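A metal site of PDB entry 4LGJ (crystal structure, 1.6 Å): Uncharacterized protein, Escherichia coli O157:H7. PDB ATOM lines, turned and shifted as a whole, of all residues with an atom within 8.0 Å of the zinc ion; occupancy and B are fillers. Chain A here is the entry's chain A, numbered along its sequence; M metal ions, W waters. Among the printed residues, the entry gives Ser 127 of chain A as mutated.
Merely in contact with the zinc ion: Tyr 205 (3.0 Å).
Within 4 Å of the zinc ion: His 161, His 165, Asp 172 and Tyr 205.
Along chain A the residues within 4 Å of the zinc ion span positions 161 to 205.
Water W1 bridges OE2 of Glu 162 (2.6 Å) and OH of Tyr 205 (3.4 Å).
The zinc ion is bound by a ring nitrogen (NE2) of His 161 (2.1 Å), the side-chain carboxylate (OD2) of Asp 172 (2.1 Å), water W1 (2.1 Å) and a ring nitrogen (NE2) of His 165 (2.2 Å).
Slightly farther from the zinc ion lies OD1 of Asp 172 (2.8 Å).
The backbone carbonyl oxygen (O) of Ser 170 is in hydrogen-bond range of a ring nitrogen (ND1) of His 165, 2.7 Å away.
A ring nitrogen (ND1) of His 165 lies close to the side-chain hydroxyl of Thr 184.
The backbone carbonyl oxygen (O) of Tyr 205 lies within hydrogen-bond range of the guanidinium group (NH2) of Arg 210, at 2.9 Å.
OD2 of Asp 172 lies close to OH of Tyr 205.
A ring nitrogen (ND1) of His 161 sits at hydrogen-bond distance from the side-chain carboxylate of Glu 185 (2.7 Å).
NE2 of His 161 lies close to OH of Tyr 205 (3.3 Å).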
ATOM      1  N   SER A 127     -13.929  -5.050 -26.059  1.00  0.00           N
ATOM      2  CA  SER A 127     -15.221  -4.765 -25.475  1.00  0.00           C
ATOM      3  C   SER A 127     -15.043  -3.794 -24.321  1.00  0.00           C
ATOM      4  O   SER A 127     -14.606  -4.182 -23.228  1.00  0.00           O
ATOM      5  CB  SER A 127     -15.895  -6.048 -24.987  1.00  0.00           C
ATOM      6  OG  SER A 127     -16.026  -6.970 -26.051  1.00  0.00           O
ATOM      7  N   GLU A 128     -15.346  -2.529 -24.556  1.00  0.00           N
ATOM      8  CA  GLU A 128     -15.118  -1.523 -23.529  1.00  0.00           C
ATOM      9  C   GLU A 128     -15.911  -0.247 -23.717  1.00  0.00           C
ATOM     10  O   GLU A 128     -16.322   0.123 -24.828  1.00  0.00           O
ATOM     11  CB  GLU A 128     -13.631  -1.198 -23.412  1.00  0.00           C
ATOM     12  CG  GLU A 128     -13.083  -0.359 -24.541  1.00  0.00           C
ATOM     13  CD  GLU A 128     -11.700   0.205 -24.232  1.00  0.00           C
ATOM     14  OE1 GLU A 128     -10.858   0.235 -25.154  1.00  0.00           O
ATOM     15  OE2 GLU A 128     -11.469   0.629 -23.085  1.00  0.00           O
ATOM     16  N   ALA A 129     -16.099   0.436 -22.596  1.00  0.00           N
ATOM     17  CA  ALA A 129     -16.740   1.732 -22.596  1.00  0.00           C
ATOM     18  C   ALA A 129     -15.646   2.762 -22.394  1.00  0.00           C
ATOM     19  O   ALA A 129     -15.081   2.892 -21.293  1.00  0.00           O
ATOM     20  CB  ALA A 129     -17.786   1.807 -21.473  1.00  0.00           C
ATOM     21  N   GLY A 158     -24.410  -8.203 -23.452  1.00  0.00           N
ATOM     22  CA  GLY A 158     -23.059  -7.673 -23.303  1.00  0.00           C
ATOM     23  C   GLY A 158     -22.934  -6.241 -23.781  1.00  0.00           C
ATOM     24  O   GLY A 158     -22.158  -5.447 -23.221  1.00  0.00           O
ATOM     25  N   HIS A 161     -24.451  -4.173 -21.131  1.00  0.00           N
ATOM     26  CA  HIS A 161     -23.423  -4.098 -20.102  1.00  0.00           C
ATOM     27  C   HIS A 161     -22.459  -2.917 -20.331  1.00  0.00           C
ATOM     28  O   HIS A 161     -22.237  -2.107 -19.428  1.00  0.00           O
ATOM     29  CB  HIS A 161     -22.667  -5.419 -20.018  1.00  0.00           C
ATOM     30  CG  HIS A 161     -21.490  -5.380 -19.115  1.00  0.00           C
ATOM     31  ND1 HIS A 161     -21.450  -6.085 -17.927  1.00  0.00           N
ATOM     32  CD2 HIS A 161     -20.312  -4.718 -19.205  1.00  0.00           C
ATOM     33  CE1 HIS A 161     -20.296  -5.860 -17.328  1.00  0.00           C
ATOM     34  NE2 HIS A 161     -19.595  -5.027 -18.087  1.00  0.00           N
ATOM     35  N   GLU A 162     -21.875  -2.819 -21.518  1.00  0.00           N
ATOM     36  CA  GLU A 162     -20.930  -1.733 -21.757  1.00  0.00           C
ATOM     37  C   GLU A 162     -21.575  -0.362 -21.663  1.00  0.00           C
ATOM     38  O   GLU A 162     -20.984   0.598 -21.130  1.00  0.00           O
ATOM     39  CB  GLU A 162     -20.216  -1.892 -23.103  1.00  0.00           C
ATOM     40  CG  GLU A 162     -19.438  -3.192 -23.267  1.00  0.00           C
ATOM     41  CD  GLU A 162     -18.353  -3.372 -22.216  1.00  0.00           C
ATOM     42  OE1 GLU A 162     -17.884  -2.364 -21.636  1.00  0.00           O
ATOM     43  OE2 GLU A 162     -17.950  -4.528 -21.972  1.00  0.00           O
ATOM     44  N   ILE A 163     -22.804  -0.247 -22.173  1.00  0.00           N
ATOM     45  CA  ILE A 163     -23.564   0.999 -22.067  1.00  0.00           C
ATOM     46  C   ILE A 163     -23.792   1.377 -20.596  1.00  0.00           C
ATOM     47  O   ILE A 163     -23.688   2.547 -20.235  1.00  0.00           O
ATOM     48  CB  ILE A 163     -24.903   0.908 -22.832  1.00  0.00           C
ATOM     49  CG1 ILE A 163     -24.640   0.826 -24.332  1.00  0.00           C
ATOM     50  CG2 ILE A 163     -25.815   2.108 -22.553  1.00  0.00           C
ATOM     51  CD1 ILE A 163     -25.874   0.434 -25.119  1.00  0.00           C
ATOM     52  N   ILE A 164     -24.067   0.384 -19.743  1.00  0.00           N
ATOM     53  CA  ILE A 164     -24.294   0.635 -18.331  1.00  0.00           C
ATOM     54  C   ILE A 164     -23.083   1.276 -17.654  1.00  0.00           C
ATOM     55  O   ILE A 164     -23.243   2.148 -16.789  1.00  0.00           O
ATOM     56  CB  ILE A 164     -24.707  -0.662 -17.594  1.00  0.00           C
ATOM     57  CG1 ILE A 164     -26.099  -1.111 -18.038  1.00  0.00           C
ATOM     58  CG2 ILE A 164     -24.688  -0.477 -16.074  1.00  0.00           C
ATOM     59  CD1 ILE A 164     -27.173  -0.118 -17.762  1.00  0.00           C
ATOM     60  N   HIS A 165     -21.875   0.899 -18.067  1.00  0.00           N
ATOM     61  CA  HIS A 165     -20.672   1.559 -17.545  1.00  0.00           C
ATOM     62  C   HIS A 165     -20.763   3.070 -17.717  1.00  0.00           C
ATOM     63  O   HIS A 165     -20.493   3.833 -16.794  1.00  0.00           O
ATOM     64  CB  HIS A 165     -19.409   1.080 -18.273  1.00  0.00           C
ATOM     65  CG  HIS A 165     -18.854  -0.204 -17.760  1.00  0.00           C
ATOM     66  ND1 HIS A 165     -18.527  -0.422 -16.427  1.00  0.00           N
ATOM     67  CD2 HIS A 165     -18.498  -1.332 -18.417  1.00  0.00           C
ATOM     68  CE1 HIS A 165     -18.031  -1.635 -16.295  1.00  0.00           C
ATOM     69  NE2 HIS A 165     -17.999  -2.204 -17.487  1.00  0.00           N
ATOM     70  N   SER A 170     -20.918   2.770 -13.245  1.00  0.00           N
ATOM     71  CA  SER A 170     -20.584   1.514 -12.568  1.00  0.00           C
ATOM     72  C   SER A 170     -19.298   0.880 -13.103  1.00  0.00           C
ATOM     73  O   SER A 170     -18.879   1.148 -14.239  1.00  0.00           O
ATOM     74  CB  SER A 170     -21.724   0.528 -12.713  1.00  0.00           C
ATOM     75  OG  SER A 170     -21.973   0.244 -14.092  1.00  0.00           O
ATOM     76  N   SER A 171     -18.683   0.041 -12.281  1.00  0.00           N
ATOM     77  CA  SER A 171     -17.491  -0.688 -12.694  1.00  0.00           C
ATOM     78  C   SER A 171     -17.710  -2.188 -12.606  1.00  0.00           C
ATOM     79  O   SER A 171     -18.795  -2.656 -12.218  1.00  0.00           O
ATOM     80  CB  SER A 171     -16.291  -0.288 -11.833  1.00  0.00           C
ATOM     81  OG  SER A 171     -16.009   1.093 -11.997  1.00  0.00           O
ATOM     82  N   ASP A 172     -16.695  -2.953 -12.986  1.00  0.00           N
ATOM     83  CA  ASP A 172     -16.693  -4.390 -12.800  1.00  0.00           C
ATOM     84  C   ASP A 172     -15.901  -4.666 -11.525  1.00  0.00           C
ATOM     85  O   ASP A 172     -15.275  -3.747 -10.992  1.00  0.00           O
ATOM     86  CB  ASP A 172     -16.047  -5.052 -14.013  1.00  0.00           C
ATOM     87  CG  ASP A 172     -16.844  -4.851 -15.261  1.00  0.00           C
ATOM     88  OD1 ASP A 172     -18.095  -4.967 -15.207  1.00  0.00           O
ATOM     89  OD2 ASP A 172     -16.212  -4.556 -16.276  1.00  0.00           O
ATOM     90  N   PRO A 173     -15.930  -5.916 -11.030  1.00  0.00           N
ATOM     91  CA  PRO A 173     -15.188  -6.203  -9.796  1.00  0.00           C
ATOM     92  C   PRO A 173     -13.703  -5.879  -9.943  1.00  0.00           C
ATOM     93  O   PRO A 173     -13.129  -6.087 -11.024  1.00  0.00           O
ATOM     94  CB  PRO A 173     -15.395  -7.706  -9.602  1.00  0.00           C
ATOM     95  CG  PRO A 173     -16.696  -7.996 -10.316  1.00  0.00           C
ATOM     96  CD  PRO A 173     -16.665  -7.099 -11.511  1.00  0.00           C
ATOM     97  N   LEU A 181     -20.688 -10.815  -9.606  1.00  0.00           N
ATOM     98  CA  LEU A 181     -20.851 -10.309 -10.969  1.00  0.00           C
ATOM     99  C   LEU A 181     -20.330  -8.885 -11.118  1.00  0.00           C
ATOM    100  O   LEU A 181     -19.906  -8.479 -12.201  1.00  0.00           O
ATOM    101  CB  LEU A 181     -22.315 -10.369 -11.411  1.00  0.00           C
ATOM    102  CG  LEU A 181     -22.887 -11.772 -11.593  1.00  0.00           C
ATOM    103  CD1 LEU A 181     -24.385 -11.700 -11.824  1.00  0.00           C
ATOM    104  CD2 LEU A 181     -22.193 -12.480 -12.735  1.00  0.00           C
ATOM    105  N   THR A 184     -22.155  -3.598 -12.726  1.00  0.00           N
ATOM    106  CA  THR A 184     -22.464  -3.401 -14.127  1.00  0.00           C
ATOM    107  C   THR A 184     -23.173  -4.633 -14.681  1.00  0.00           C
ATOM    108  O   THR A 184     -24.219  -4.527 -15.329  1.00  0.00           O
ATOM    109  CB  THR A 184     -21.205  -3.142 -14.963  1.00  0.00           C
ATOM    110  OG1 THR A 184     -20.450  -2.073 -14.368  1.00  0.00           O
ATOM    111  CG2 THR A 184     -21.555  -2.737 -16.387  1.00  0.00           C
ATOM    112  N   GLU A 185     -22.610  -5.792 -14.396  1.00  0.00           N
ATOM    113  CA  GLU A 185     -23.180  -7.054 -14.881  1.00  0.00           C
ATOM    114  C   GLU A 185     -24.483  -7.404 -14.154  1.00  0.00           C
ATOM    115  O   GLU A 185     -25.401  -7.974 -14.772  1.00  0.00           O
ATOM    116  CB  GLU A 185     -22.162  -8.186 -14.843  1.00  0.00           C
ATOM    117  CG  GLU A 185     -22.658  -9.513 -15.426  1.00  0.00           C
ATOM    118  CD  GLU A 185     -22.986  -9.447 -16.914  1.00  0.00           C
ATOM    119  OE1 GLU A 185     -22.719  -8.428 -17.599  1.00  0.00           O
ATOM    120  OE2 GLU A 185     -23.528 -10.456 -17.412  1.00  0.00           O
ATOM    121  N   TYR A 205     -18.081 -12.736 -12.548  1.00  0.00           N
ATOM    122  CA  TYR A 205     -17.705 -11.978 -13.735  1.00  0.00           C
ATOM    123  C   TYR A 205     -16.536 -12.614 -14.485  1.00  0.00           C
ATOM    124  O   TYR A 205     -16.424 -12.501 -15.710  1.00  0.00           O
ATOM    125  CB  TYR A 205     -17.393 -10.523 -13.377  1.00  0.00           C
ATOM    126  CG  TYR A 205     -17.330  -9.628 -14.589  1.00  0.00           C
ATOM    127  CD1 TYR A 205     -18.482  -9.343 -15.317  1.00  0.00           C
ATOM    128  CD2 TYR A 205     -16.136  -9.080 -15.008  1.00  0.00           C
ATOM    129  CE1 TYR A 205     -18.436  -8.549 -16.448  1.00  0.00           C
ATOM    130  CE2 TYR A 205     -16.064  -8.270 -16.130  1.00  0.00           C
ATOM    131  CZ  TYR A 205     -17.230  -8.007 -16.847  1.00  0.00           C
ATOM    132  OH  TYR A 205     -17.174  -7.211 -17.963  1.00  0.00           O
ATOM    133  N   ARG A 210     -17.921 -18.500 -17.851  1.00  0.00           N
ATOM    134  CA  ARG A 210     -18.337 -17.223 -18.449  1.00  0.00           C
ATOM    135  C   ARG A 210     -17.306 -16.795 -19.488  1.00  0.00           C
ATOM    136  O   ARG A 210     -17.659 -16.440 -20.625  1.00  0.00           O
ATOM    137  CB  ARG A 210     -18.540 -16.131 -17.377  1.00  0.00           C
ATOM    138  CG  ARG A 210     -18.949 -14.782 -17.988  1.00  0.00           C
ATOM    139  CD  ARG A 210     -19.369 -13.737 -16.960  1.00  0.00           C
ATOM    140  NE  ARG A 210     -19.953 -12.615 -17.677  1.00  0.00           N
ATOM    141  CZ  ARG A 210     -19.267 -11.583 -18.168  1.00  0.00           C
ATOM    142  NH1 ARG A 210     -19.895 -10.640 -18.854  1.00  0.00           N
ATOM    143  NH2 ARG A 210     -17.947 -11.479 -17.970  1.00  0.00           N
HETATM  144 ZN    ZN M   1     -17.624  -4.296 -17.843  1.00  0.00          ZN
HETATM  145  O   HOH W   1     -16.577  -4.417 -19.715  1.00  0.00           O
